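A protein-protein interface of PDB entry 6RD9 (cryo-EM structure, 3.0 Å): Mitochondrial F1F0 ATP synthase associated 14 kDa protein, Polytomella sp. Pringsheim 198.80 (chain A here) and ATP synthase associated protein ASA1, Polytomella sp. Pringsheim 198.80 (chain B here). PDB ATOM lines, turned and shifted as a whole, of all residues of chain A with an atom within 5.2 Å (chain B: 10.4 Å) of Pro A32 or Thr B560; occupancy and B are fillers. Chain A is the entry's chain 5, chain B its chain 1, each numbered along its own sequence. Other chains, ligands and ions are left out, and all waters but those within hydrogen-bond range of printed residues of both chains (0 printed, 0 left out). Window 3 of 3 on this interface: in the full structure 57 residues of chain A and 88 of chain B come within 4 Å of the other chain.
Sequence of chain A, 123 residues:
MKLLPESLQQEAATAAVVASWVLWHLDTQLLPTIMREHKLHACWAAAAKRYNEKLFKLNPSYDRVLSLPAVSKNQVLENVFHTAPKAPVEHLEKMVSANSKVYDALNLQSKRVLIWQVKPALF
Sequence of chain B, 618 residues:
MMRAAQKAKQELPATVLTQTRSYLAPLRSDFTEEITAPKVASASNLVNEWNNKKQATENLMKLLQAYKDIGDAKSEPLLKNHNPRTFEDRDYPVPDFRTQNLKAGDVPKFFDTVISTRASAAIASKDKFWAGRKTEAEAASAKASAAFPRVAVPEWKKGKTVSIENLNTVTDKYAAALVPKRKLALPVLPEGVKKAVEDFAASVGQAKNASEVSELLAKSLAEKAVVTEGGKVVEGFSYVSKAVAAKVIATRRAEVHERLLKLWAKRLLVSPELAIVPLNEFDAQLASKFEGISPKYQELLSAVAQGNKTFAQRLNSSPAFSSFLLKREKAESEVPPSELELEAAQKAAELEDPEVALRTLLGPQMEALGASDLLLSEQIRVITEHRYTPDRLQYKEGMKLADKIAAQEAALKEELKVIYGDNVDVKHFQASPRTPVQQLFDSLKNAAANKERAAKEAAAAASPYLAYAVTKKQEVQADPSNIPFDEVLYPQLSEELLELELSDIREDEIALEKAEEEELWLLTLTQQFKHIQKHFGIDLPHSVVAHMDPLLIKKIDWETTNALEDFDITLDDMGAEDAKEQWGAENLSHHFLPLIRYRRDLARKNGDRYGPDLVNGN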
ATOM      1  N   LEU A  26     -23.415 -15.262  -0.784  1.00  0.00           N
ATOM      2  CA  LEU A  26     -24.182 -15.302   0.442  1.00  0.00           C
ATOM      3  C   LEU A  26     -23.426 -16.035   1.533  1.00  0.00           C
ATOM      4  O   LEU A  26     -23.305 -15.534   2.643  1.00  0.00           O
ATOM      5  CB  LEU A  26     -25.503 -15.973   0.168  1.00  0.00           C
ATOM      6  CG  LEU A  26     -26.560 -16.057   1.212  1.00  0.00           C
ATOM      7  CD1 LEU A  26     -27.244 -14.754   1.261  1.00  0.00           C
ATOM      8  CD2 LEU A  26     -27.443 -17.114   0.723  1.00  0.00           C
ATOM      9  N   ASP A  27     -22.888 -17.208   1.228  1.00  0.00           N
ATOM     10  CA  ASP A  27     -22.244 -18.035   2.238  1.00  0.00           C
ATOM     11  C   ASP A  27     -20.952 -17.459   2.743  1.00  0.00           C
ATOM     12  O   ASP A  27     -20.549 -17.749   3.865  1.00  0.00           O
ATOM     13  CB  ASP A  27     -21.904 -19.382   1.676  1.00  0.00           C
ATOM     14  CG  ASP A  27     -22.932 -20.388   1.923  1.00  0.00           C
ATOM     15  OD1 ASP A  27     -23.666 -20.275   2.912  1.00  0.00           O
ATOM     16  OD2 ASP A  27     -22.956 -21.356   1.160  1.00  0.00           O
ATOM     17  N   THR A  28     -20.260 -16.710   1.916  1.00  0.00           N
ATOM     18  CA  THR A  28     -18.922 -16.248   2.208  1.00  0.00           C
ATOM     19  C   THR A  28     -18.904 -14.794   2.635  1.00  0.00           C
ATOM     20  O   THR A  28     -18.252 -14.446   3.606  1.00  0.00           O
ATOM     21  CB  THR A  28     -18.059 -16.478   0.979  1.00  0.00           C
ATOM     22  OG1 THR A  28     -17.764 -17.861   0.867  1.00  0.00           O
ATOM     23  CG2 THR A  28     -16.822 -15.740   1.022  1.00  0.00           C
ATOM     24  N   GLN A  29     -19.646 -13.939   1.954  1.00  0.00           N
ATOM     25  CA  GLN A  29     -19.595 -12.517   2.221  1.00  0.00           C
ATOM     26  C   GLN A  29     -20.785 -12.007   3.003  1.00  0.00           C
ATOM     27  O   GLN A  29     -20.605 -11.256   3.955  1.00  0.00           O
ATOM     28  CB  GLN A  29     -19.471 -11.750   0.914  1.00  0.00           C
ATOM     29  CG  GLN A  29     -18.470 -12.343  -0.025  1.00  0.00           C
ATOM     30  CD  GLN A  29     -17.076 -12.008   0.351  1.00  0.00           C
ATOM     31  OE1 GLN A  29     -16.139 -12.714   0.017  1.00  0.00           O
ATOM     32  NE2 GLN A  29     -16.911 -10.906   1.055  1.00  0.00           N
ATOM     33  N   LEU A  30     -21.995 -12.390   2.634  1.00  0.00           N
ATOM     34  CA  LEU A  30     -23.152 -11.848   3.329  1.00  0.00           C
ATOM     35  C   LEU A  30     -23.383 -12.526   4.664  1.00  0.00           C
ATOM     36  O   LEU A  30     -23.443 -11.854   5.685  1.00  0.00           O
ATOM     37  CB  LEU A  30     -24.390 -11.960   2.463  1.00  0.00           C
ATOM     38  CG  LEU A  30     -24.356 -11.137   1.199  1.00  0.00           C
ATOM     39  CD1 LEU A  30     -25.683 -11.223   0.565  1.00  0.00           C
ATOM     40  CD2 LEU A  30     -24.021  -9.724   1.496  1.00  0.00           C
ATOM     41  N   LEU A  31     -23.499 -13.850   4.689  1.00  0.00           N
ATOM     42  CA  LEU A  31     -23.885 -14.524   5.924  1.00  0.00           C
ATOM     43  C   LEU A  31     -22.858 -14.509   7.048  1.00  0.00           C
ATOM     44  O   LEU A  31     -23.286 -14.661   8.200  1.00  0.00           O
ATOM     45  CB  LEU A  31     -24.264 -15.978   5.662  1.00  0.00           C
ATOM     46  CG  LEU A  31     -25.679 -16.380   5.325  1.00  0.00           C
ATOM     47  CD1 LEU A  31     -25.699 -17.863   5.236  1.00  0.00           C
ATOM     48  CD2 LEU A  31     -26.579 -15.899   6.399  1.00  0.00           C
ATOM     49  N   PRO A  32     -21.550 -14.414   6.824  1.00  0.00           N
ATOM     50  CA  PRO A  32     -20.677 -14.076   7.939  1.00  0.00           C
ATOM     51  C   PRO A  32     -20.931 -12.721   8.543  1.00  0.00           C
ATOM     52  O   PRO A  32     -20.852 -12.587   9.757  1.00  0.00           O
ATOM     53  CB  PRO A  32     -19.305 -14.174   7.296  1.00  0.00           C
ATOM     54  CG  PRO A  32     -19.459 -15.281   6.469  1.00  0.00           C
ATOM     55  CD  PRO A  32     -20.758 -15.149   5.834  1.00  0.00           C
ATOM     56  N   THR A  33     -21.246 -11.721   7.746  1.00  0.00           N
ATOM     57  CA  THR A  33     -21.586 -10.401   8.239  1.00  0.00           C
ATOM     58  C   THR A  33     -22.945 -10.363   8.917  1.00  0.00           C
ATOM     59  O   THR A  33     -23.112  -9.650   9.906  1.00  0.00           O
ATOM     60  CB  THR A  33     -21.553  -9.443   7.066  1.00  0.00           C
ATOM     61  OG1 THR A  33     -20.265  -9.509   6.459  1.00  0.00           O
ATOM     62  CG2 THR A  33     -21.820  -8.068   7.489  1.00  0.00           C
ATOM     63  N   ILE A  34     -23.921 -11.107   8.391  1.00  0.00           N
ATOM     64  CA  ILE A  34     -25.237 -11.210   9.016  1.00  0.00           C
ATOM     65  C   ILE A  34     -25.100 -11.767  10.411  1.00  0.00           C
ATOM     66  O   ILE A  34     -25.606 -11.200  11.373  1.00  0.00           O
ATOM     67  CB  ILE A  34     -26.172 -12.103   8.183  1.00  0.00           C
ATOM     68  CG1 ILE A  34     -26.456 -11.549   6.802  1.00  0.00           C
ATOM     69  CG2 ILE A  34     -27.448 -12.364   8.900  1.00  0.00           C
ATOM     70  CD1 ILE A  34     -26.947 -10.246   6.786  1.00  0.00           C
ATOM     71  N   MET A  35     -24.385 -12.869  10.543  1.00  0.00           N
ATOM     72  CA  MET A  35     -24.300 -13.582  11.798  1.00  0.00           C
ATOM     73  C   MET A  35     -23.333 -12.951  12.765  1.00  0.00           C
ATOM     74  O   MET A  35     -23.376 -13.277  13.938  1.00  0.00           O
ATOM     75  CB  MET A  35     -23.893 -15.021  11.555  1.00  0.00           C
ATOM     76  CG  MET A  35     -24.920 -15.834  10.879  1.00  0.00           C
ATOM     77  SD  MET A  35     -26.538 -15.535  11.532  1.00  0.00           S
ATOM     78  CE  MET A  35     -27.483 -16.046  10.142  1.00  0.00           C
ATOM     79  N   ARG A  36     -22.467 -12.064  12.325  1.00  0.00           N
ATOM     80  CA  ARG A  36     -21.597 -11.406  13.275  1.00  0.00           C
ATOM     81  C   ARG A  36     -22.350 -10.359  14.046  1.00  0.00           C
ATOM     82  O   ARG A  36     -22.028 -10.082  15.196  1.00  0.00           O
ATOM     83  CB  ARG A  36     -20.420 -10.781  12.566  1.00  0.00           C
ATOM     84  CG  ARG A  36     -19.250 -11.655  12.499  1.00  0.00           C
ATOM     85  CD  ARG A  36     -18.225 -11.007  11.684  1.00  0.00           C
ATOM     86  NE  ARG A  36     -17.139 -11.907  11.385  1.00  0.00           N
ATOM     87  CZ  ARG A  36     -15.912 -11.491  11.157  1.00  0.00           C
ATOM     88  NH1 ARG A  36     -14.957 -12.355  10.903  1.00  0.00           N
ATOM     89  NH2 ARG A  36     -15.652 -10.205  11.209  1.00  0.00           N
ATOM     90  N   LYS A  39     -25.603 -12.357  15.985  1.00  0.00           N
ATOM     91  CA  LYS A  39     -25.230 -13.120  17.156  1.00  0.00           C
ATOM     92  C   LYS A  39     -24.429 -12.342  18.174  1.00  0.00           C
ATOM     93  O   LYS A  39     -24.196 -12.867  19.249  1.00  0.00           O
ATOM     94  CB  LYS A  39     -24.438 -14.341  16.755  1.00  0.00           C
ATOM     95  CG  LYS A  39     -25.231 -15.292  15.982  1.00  0.00           C
ATOM     96  CD  LYS A  39     -24.418 -16.428  15.563  1.00  0.00           C
ATOM     97  CE  LYS A  39     -25.298 -17.450  14.977  1.00  0.00           C
ATOM     98  NZ  LYS A  39     -24.447 -18.485  14.452  1.00  0.00           N
ATOM     99  N   HIS B 542     -17.829  -3.124  11.813  1.00  0.00           N
ATOM    100  CA  HIS B 542     -17.509  -4.481  12.186  1.00  0.00           C
ATOM    101  C   HIS B 542     -16.062  -4.661  12.563  1.00  0.00           C
ATOM    102  O   HIS B 542     -15.719  -5.688  13.141  1.00  0.00           O
ATOM    103  CB  HIS B 542     -17.831  -5.405  11.039  1.00  0.00           C
ATOM    104  CG  HIS B 542     -19.225  -5.920  11.048  1.00  0.00           C
ATOM    105  ND1 HIS B 542     -20.299  -5.138  10.719  1.00  0.00           N
ATOM    106  CD2 HIS B 542     -19.712  -7.154  11.260  1.00  0.00           C
ATOM    107  CE1 HIS B 542     -21.397  -5.857  10.773  1.00  0.00           C
ATOM    108  NE2 HIS B 542     -21.067  -7.087  11.095  1.00  0.00           N
ATOM    109  N   VAL B 545     -15.938  -3.934  16.464  1.00  0.00           N
ATOM    110  CA  VAL B 545     -16.464  -5.060  17.223  1.00  0.00           C
ATOM    111  C   VAL B 545     -15.429  -6.162  17.319  1.00  0.00           C
ATOM    112  O   VAL B 545     -15.172  -6.706  18.391  1.00  0.00           O
ATOM    113  CB  VAL B 545     -17.744  -5.577  16.565  1.00  0.00           C
ATOM    114  CG1 VAL B 545     -18.167  -6.809  17.209  1.00  0.00           C
ATOM    115  CG2 VAL B 545     -18.793  -4.588  16.654  1.00  0.00           C
ATOM    116  N   ALA B 546     -14.804  -6.499  16.205  1.00  0.00           N
ATOM    117  CA  ALA B 546     -13.804  -7.546  16.207  1.00  0.00           C
ATOM    118  C   ALA B 546     -12.513  -7.103  16.839  1.00  0.00           C
ATOM    119  O   ALA B 546     -11.656  -7.939  17.112  1.00  0.00           O
ATOM    120  CB  ALA B 546     -13.540  -8.008  14.790  1.00  0.00           C
ATOM    121  N   LEU B 552     -15.349 -13.177  20.684  1.00  0.00           N
ATOM    122  CA  LEU B 552     -16.755 -13.355  20.366  1.00  0.00           C
ATOM    123  C   LEU B 552     -16.932 -13.524  18.882  1.00  0.00           C
ATOM    124  O   LEU B 552     -17.699 -14.370  18.435  1.00  0.00           O
ATOM    125  CB  LEU B 552     -17.569 -12.169  20.845  1.00  0.00           C
ATOM    126  CG  LEU B 552     -19.049 -12.237  20.539  1.00  0.00           C
ATOM    127  CD1 LEU B 552     -19.670 -13.362  21.260  1.00  0.00           C
ATOM    128  CD2 LEU B 552     -19.708 -10.988  20.901  1.00  0.00           C
ATOM    129  N   ILE B 553     -16.206 -12.734  18.105  1.00  0.00           N
ATOM    130  CA  ILE B 553     -16.174 -12.863  16.661  1.00  0.00           C
ATOM    131  C   ILE B 553     -15.556 -14.182  16.251  1.00  0.00           C
ATOM    132  O   ILE B 553     -15.999 -14.795  15.289  1.00  0.00           O
ATOM    133  CB  ILE B 553     -15.423 -11.647  16.108  1.00  0.00           C
ATOM    134  CG1 ILE B 553     -16.214 -10.385  16.393  1.00  0.00           C
ATOM    135  CG2 ILE B 553     -15.119 -11.765  14.683  1.00  0.00           C
ATOM    136  CD1 ILE B 553     -17.599 -10.414  15.917  1.00  0.00           C
ATOM    137  N   LYS B 554     -14.575 -14.672  16.996  1.00  0.00           N
ATOM    138  CA  LYS B 554     -13.951 -15.955  16.710  1.00  0.00           C
ATOM    139  C   LYS B 554     -14.914 -17.107  16.908  1.00  0.00           C
ATOM    140  O   LYS B 554     -14.906 -18.061  16.136  1.00  0.00           O
ATOM    141  CB  LYS B 554     -12.739 -16.141  17.604  1.00  0.00           C
ATOM    142  CG  LYS B 554     -11.951 -17.372  17.339  1.00  0.00           C
ATOM    143  CD  LYS B 554     -11.236 -17.800  18.556  1.00  0.00           C
ATOM    144  CE  LYS B 554     -10.460 -19.026  18.309  1.00  0.00           C
ATOM    145  NZ  LYS B 554      -9.940 -19.538  19.582  1.00  0.00           N
ATOM    146  N   LYS B 555     -15.753 -17.040  17.931  1.00  0.00           N
ATOM    147  CA  LYS B 555     -16.719 -18.093  18.184  1.00  0.00           C
ATOM    148  C   LYS B 555     -17.947 -17.977  17.309  1.00  0.00           C
ATOM    149  O   LYS B 555     -18.606 -18.977  17.062  1.00  0.00           O
ATOM    150  CB  LYS B 555     -17.159 -18.059  19.630  1.00  0.00           C
ATOM    151  CG  LYS B 555     -16.109 -18.380  20.597  1.00  0.00           C
ATOM    152  CD  LYS B 555     -16.666 -18.352  21.955  1.00  0.00           C
ATOM    153  CE  LYS B 555     -15.720 -17.759  22.889  1.00  0.00           C
ATOM    154  NZ  LYS B 555     -16.069 -18.150  24.240  1.00  0.00           N
ATOM    155  N   ILE B 556     -18.316 -16.770  16.900  1.00  0.00           N
ATOM    156  CA  ILE B 556     -19.386 -16.591  15.928  1.00  0.00           C
ATOM    157  C   ILE B 556     -18.971 -17.147  14.583  1.00  0.00           C
ATOM    158  O   ILE B 556     -19.743 -17.836  13.919  1.00  0.00           O
ATOM    159  CB  ILE B 556     -19.759 -15.105  15.837  1.00  0.00           C
ATOM    160  CG1 ILE B 556     -20.639 -14.692  16.996  1.00  0.00           C
ATOM    161  CG2 ILE B 556     -20.479 -14.808  14.602  1.00  0.00           C
ATOM    162  CD1 ILE B 556     -20.726 -13.248  17.130  1.00  0.00           C
ATOM    163  N   ASP B 557     -17.731 -16.897  14.181  1.00  0.00           N
ATOM    164  CA  ASP B 557     -17.197 -17.435  12.943  1.00  0.00           C
ATOM    165  C   ASP B 557     -17.049 -18.933  12.965  1.00  0.00           C
ATOM    166  O   ASP B 557     -16.924 -19.533  11.908  1.00  0.00           O
ATOM    167  CB  ASP B 557     -15.831 -16.852  12.655  1.00  0.00           C
ATOM    168  CG  ASP B 557     -15.887 -15.429  12.268  1.00  0.00           C
ATOM    169  OD1 ASP B 557     -16.985 -14.868  12.262  1.00  0.00           O
ATOM    170  OD2 ASP B 557     -14.829 -14.867  11.961  1.00  0.00           O
ATOM    171  N   TRP B 558     -16.991 -19.550  14.132  1.00  0.00           N
ATOM    172  CA  TRP B 558     -16.949 -21.000  14.173  1.00  0.00           C
ATOM    173  C   TRP B 558     -18.287 -21.585  13.789  1.00  0.00           C
ATOM    174  O   TRP B 558     -18.345 -22.650  13.189  1.00  0.00           O
ATOM    175  CB  TRP B 558     -16.534 -21.490  15.552  1.00  0.00           C
ATOM    176  CG  TRP B 558     -16.349 -22.953  15.617  1.00  0.00           C
ATOM    177  CD1 TRP B 558     -15.215 -23.624  15.400  1.00  0.00           C
ATOM    178  CD2 TRP B 558     -17.345 -23.930  15.911  1.00  0.00           C
ATOM    179  NE1 TRP B 558     -15.429 -24.959  15.534  1.00  0.00           N
ATOM    180  CE2 TRP B 558     -16.737 -25.162  15.855  1.00  0.00           C
ATOM    181  CE3 TRP B 558     -18.698 -23.871  16.216  1.00  0.00           C
ATOM    182  CZ2 TRP B 558     -17.424 -26.315  16.065  1.00  0.00           C
ATOM    183  CZ3 TRP B 558     -19.363 -24.996  16.423  1.00  0.00           C
ATOM    184  CH2 TRP B 558     -18.742 -26.207  16.353  1.00  0.00           C
ATOM    185  N   GLU B 559     -19.373 -20.920  14.141  1.00  0.00           N
ATOM    186  CA  GLU B 559     -20.681 -21.426  13.773  1.00  0.00           C
ATOM    187  C   GLU B 559     -20.934 -21.272  12.289  1.00  0.00           C
ATOM    188  O   GLU B 559     -21.594 -22.111  11.687  1.00  0.00           O
ATOM    189  CB  GLU B 559     -21.745 -20.700  14.553  1.00  0.00           C
ATOM    190  CG  GLU B 559     -21.477 -20.657  15.979  1.00  0.00           C
ATOM    191  CD  GLU B 559     -22.678 -20.272  16.755  1.00  0.00           C
ATOM    192  OE1 GLU B 559     -23.777 -20.364  16.208  1.00  0.00           O
ATOM    193  OE2 GLU B 559     -22.536 -19.865  17.912  1.00  0.00           O
ATOM    194  N   THR B 560     -20.450 -20.198  11.684  1.00  0.00           N
ATOM    195  CA  THR B 560     -20.611 -20.047  10.250  1.00  0.00           C
ATOM    196  C   THR B 560     -19.735 -21.028   9.500  1.00  0.00           C
ATOM    197  O   THR B 560     -20.154 -21.578   8.488  1.00  0.00           O
ATOM    198  CB  THR B 560     -20.296 -18.621   9.832  1.00  0.00           C
ATOM    199  OG1 THR B 560     -20.980 -17.722  10.696  1.00  0.00           O
ATOM    200  CG2 THR B 560     -20.767 -18.365   8.471  1.00  0.00           C
ATOM    201  N   THR B 561     -18.531 -21.282   9.997  1.00  0.00           N
ATOM    202  CA  THR B 561     -17.631 -22.208   9.329  1.00  0.00           C
ATOM    203  C   THR B 561     -18.140 -23.626   9.421  1.00  0.00           C
ATOM    204  O   THR B 561     -18.100 -24.376   8.448  1.00  0.00           O
ATOM    205  CB  THR B 561     -16.253 -22.106   9.944  1.00  0.00           C
ATOM    206  OG1 THR B 561     -15.815 -20.757   9.868  1.00  0.00           O
ATOM    207  CG2 THR B 561     -15.284 -22.947   9.227  1.00  0.00           C
ATOM    208  N   ASN B 562     -18.665 -23.995  10.575  1.00  0.00           N
ATOM    209  CA  ASN B 562     -19.128 -25.344  10.829  1.00  0.00           C
ATOM    210  C   ASN B 562     -20.615 -25.480  10.674  1.00  0.00           C
ATOM    211  O   ASN B 562     -21.235 -26.230  11.421  1.00  0.00           O
ATOM    212  CB  ASN B 562     -18.697 -25.775  12.210  1.00  0.00           C
ATOM    213  CG  ASN B 562     -17.238 -25.864  12.307  1.00  0.00           C
ATOM    214  OD1 ASN B 562     -16.578 -24.883  12.545  1.00  0.00           O
ATOM    215  ND2 ASN B 562     -16.702 -27.029  12.064  1.00  0.00           N
ATOM    216  N   ALA B 563     -21.190 -24.716   9.758  1.00  0.00           N
ATOM    217  CA  ALA B 563     -22.520 -24.908   9.204  1.00  0.00           C
ATOM    218  C   ALA B 563     -23.618 -24.817  10.235  1.00  0.00           C
ATOM    219  O   ALA B 563     -24.684 -25.391  10.054  1.00  0.00           O
ATOM    220  CB  ALA B 563     -22.612 -26.234   8.465  1.00  0.00           C
ATOM    221  N   LEU B 564     -23.375 -24.126  11.327  1.00  0.00           N
ATOM    222  CA  LEU B 564     -24.362 -23.922  12.369  1.00  0.00           C
ATOM    223  C   LEU B 564     -24.718 -22.457  12.475  1.00  0.00           C
ATOM    224  O   LEU B 564     -24.929 -21.944  13.563  1.00  0.00           O
ATOM    225  CB  LEU B 564     -23.853 -24.404  13.714  1.00  0.00           C
ATOM    226  CG  LEU B 564     -23.411 -25.830  13.949  1.00  0.00           C
ATOM    227  CD1 LEU B 564     -22.609 -25.821  15.183  1.00  0.00           C
ATOM    228  CD2 LEU B 564     -24.601 -26.679  14.146  1.00  0.00           C
ATOM    229  N   GLU B 565     -24.796 -21.763  11.343  1.00  0.00           N
ATOM    230  CA  GLU B 565     -25.100 -20.343  11.375  1.00  0.00           C
ATOM    231  C   GLU B 565     -26.534 -20.066  11.768  1.00  0.00           C
ATOM    232  O   GLU B 565     -26.881 -18.918  12.030  1.00  0.00           O
ATOM    233  CB  GLU B 565     -24.814 -19.694  10.029  1.00  0.00           C
ATOM    234  CG  GLU B 565     -25.739 -20.119   8.944  1.00  0.00           C
ATOM    235  CD  GLU B 565     -25.198 -21.257   8.144  1.00  0.00           C
ATOM    236  OE1 GLU B 565     -24.146 -21.791   8.521  1.00  0.00           O
ATOM    237  OE2 GLU B 565     -25.827 -21.640   7.145  1.00  0.00           O
ATOM    238  N   ASP B 566     -27.379 -21.075  11.817  1.00  0.00           N
ATOM    239  CA  ASP B 566     -28.729 -20.930  12.311  1.00  0.00           C
ATOM    240  C   ASP B 566     -28.933 -21.662  13.623  1.00  0.00           C
ATOM    241  O   ASP B 566     -30.028 -22.143  13.884  1.00  0.00           O
ATOM    242  CB  ASP B 566     -29.714 -21.442  11.277  1.00  0.00           C
ATOM    243  CG  ASP B 566     -29.459 -22.869  10.899  1.00  0.00           C
ATOM    244  OD1 ASP B 566     -28.290 -23.273  10.832  1.00  0.00           O
ATOM    245  OD2 ASP B 566     -30.433 -23.597  10.660  1.00  0.00           O
ATOM    246  N   PHE B 567     -27.901 -21.755  14.460  1.00  0.00           N
ATOM    247  CA  PHE B 567     -28.009 -22.583  15.652  1.00  0.00           C
ATOM    248  C   PHE B 567     -28.939 -21.981  16.679  1.00  0.00           C
ATOM    249  O   PHE B 567     -29.617 -22.715  17.389  1.00  0.00           O
ATOM    250  CB  PHE B 567     -26.649 -22.821  16.281  1.00  0.00           C
ATOM    251  CG  PHE B 567     -26.668 -23.847  17.362  1.00  0.00           C
ATOM    252  CD1 PHE B 567     -27.104 -25.125  17.101  1.00  0.00           C
ATOM    253  CD2 PHE B 567     -26.243 -23.543  18.631  1.00  0.00           C
ATOM    254  CE1 PHE B 567     -27.127 -26.074  18.089  1.00  0.00           C
ATOM    255  CE2 PHE B 567     -26.264 -24.483  19.615  1.00  0.00           C
ATOM    256  CZ  PHE B 567     -26.700 -25.749  19.344  1.00  0.00           C
ATOM    257  N   ASP B 568     -29.011 -20.667  16.765  1.00  0.00           N
ATOM    258  CA  ASP B 568     -30.005 -20.085  17.640  1.00  0.00           C
ATOM    259  C   ASP B 568     -31.406 -20.143  17.058  1.00  0.00           C
ATOM    260  O   ASP B 568     -32.372 -19.967  17.798  1.00  0.00           O
ATOM    261  CB  ASP B 568     -29.639 -18.651  17.973  1.00  0.00           C
ATOM    262  CG  ASP B 568     -29.835 -17.717  16.829  1.00  0.00           C
ATOM    263  OD1 ASP B 568     -29.179 -17.882  15.792  1.00  0.00           O
ATOM    264  OD2 ASP B 568     -30.653 -16.796  16.974  1.00  0.00           O
ATOM    265  N   TRP B 583     -26.210 -21.159  25.323  1.00  0.00           N
ATOM    266  CA  TRP B 583     -25.498 -20.812  24.104  1.00  0.00           C
ATOM    267  C   TRP B 583     -24.993 -19.392  24.166  1.00  0.00           C
ATOM    268  O   TRP B 583     -23.862 -19.117  23.771  1.00  0.00           O
ATOM    269  CB  TRP B 583     -26.405 -21.005  22.897  1.00  0.00           C
ATOM    270  CG  TRP B 583     -25.938 -20.355  21.644  1.00  0.00           C
ATOM    271  CD1 TRP B 583     -25.026 -20.830  20.771  1.00  0.00           C
ATOM    272  CD2 TRP B 583     -26.384 -19.118  21.116  1.00  0.00           C
ATOM    273  NE1 TRP B 583     -24.855 -19.962  19.748  1.00  0.00           N
ATOM    274  CE2 TRP B 583     -25.683 -18.895  19.942  1.00  0.00           C
ATOM    275  CE3 TRP B 583     -27.295 -18.160  21.542  1.00  0.00           C
ATOM    276  CZ2 TRP B 583     -25.875 -17.775  19.179  1.00  0.00           C
ATOM    277  CZ3 TRP B 583     -27.479 -17.065  20.787  1.00  0.00           C
ATOM    278  CH2 TRP B 583     -26.785 -16.878  19.613  1.00  0.00           C
ATOM    279  N   ASN B 587     -20.764 -18.114  24.901  1.00  0.00           N
ATOM    280  CA  ASN B 587     -20.119 -17.330  23.870  1.00  0.00           C
ATOM    281  C   ASN B 587     -19.579 -16.030  24.390  1.00  0.00           C
ATOM    282  O   ASN B 587     -18.754 -15.408  23.725  1.00  0.00           O
ATOM    283  CB  ASN B 587     -21.085 -17.027  22.737  1.00  0.00           C
ATOM    284  CG  ASN B 587     -21.172 -18.134  21.742  1.00  0.00           C
ATOM    285  OD1 ASN B 587     -21.990 -18.103  20.847  1.00  0.00           O
ATOM    286  ND2 ASN B 587     -20.328 -19.126  21.891  1.00  0.00           N
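CG2 of Thr B560 touches CG of Pro A32, at 3.9 Å. Met A35 touches Ile B556. CD2 of His B542 touches CB of Arg A36 (3.9 Å). CZ of Arg A36 touches CG2 of Ile B553, 3.6 Å away. CG2 of Ile B556 touches CA of Arg A36, at 3.8 Å. CB of Lys A39 touches CG1 of Ile B556 (3.8 Å). NZ of Lys A39 touches O of Leu B564 (3.6 Å). CE of Lys A39 touches OD1 of Asp B568, at 3.99 Å.
The backbone carbonyl oxygen (O) of Ile B556 lies within hydrogen-bond range of the side-chain hydroxyl (OG1) of Thr B560 (3.5 Å). O of Asp B557 sits at hydrogen-bond distance from OG1 of Thr B561 (2.6 Å). The backbone NH of Leu B564 sits at hydrogen-bond distance from the backbone carbonyl oxygen of Glu B559 (2.7 Å). N of Glu B565 sits at hydrogen-bond distance from O of Glu B559 (3.2 Å). The side-chain carboxylate (OE2) of Glu B559 lies close to the side-chain amide oxygen (OD1) of Asn B587 (3.5 Å). OG1 of Thr A33 lies within hydrogen-bond range of O of Gln A29 (3.1 Å).
No residue of chain B comes within 4 Å of Leu A31. Pro A32 touches just one residue of chain B: Thr B560 (3.9 Å). Of chain B, only His B542 comes within 4 Å of Thr A33. Of the printed residues of chain B, Arg A36 touches His B542 (3.9 Å), Ile B553 (3.6 Å), Ile B556 (3.8 Å) and Asp B557 (2.7 Å). Of the printed residues of chain A, His B542 touches Thr A33 (3.5 Å) and Arg A36 (3.9 Å). Of the printed residues of chain A, Ile B553 touches Arg A36. Printed residues of chain A within 4 Å of Asp B557: Arg A36 (2.7 Å). Thr B560 touches just one residue of chain A: Pro A32. Printed residues of chain A within 4 Å of Glu B565: Met A35 and Lys A39. The nearest residue of chain B that does not touch Pro A32 is Asp B557 (5.1 Å). The nearest residue of chain A that does not touch Thr B560 is Met A35 (4.1 Å).
Of the 22 printed residues of chain B, 9 touch a printed residue of chain A. Printed residues of chain B that touch a printed residue of chain A: His B542, Ile B553, Ile B556, Asp B557, Glu B559, Thr B560, Leu B564, Glu B565 and Asp B568. Hydrophobic or aromatic side chains of chain B within 4 Å of the printed part of chain A: His B542, Ile B553 and Ile B556. Along chain A the printed residues that touch a printed residue of chain B span positions 32 to 39.
NE2 of His B542 sits at hydrogen-bond distance from O of Thr A33. The side-chain carboxylate (OD2) of Asp B557 is in salt-bridge range of the guanidinium group (NH1) of Arg A36 (2.7 Å). The side-chain amino group of Lys A39 lies within salt-bridge range of the side-chain carboxylate of Glu B559. O of Glu B565 is in hydrogen-bond range of NZ of Lys A39. SD of Met A35 lies close to O of Glu B565 (3.4 Å).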
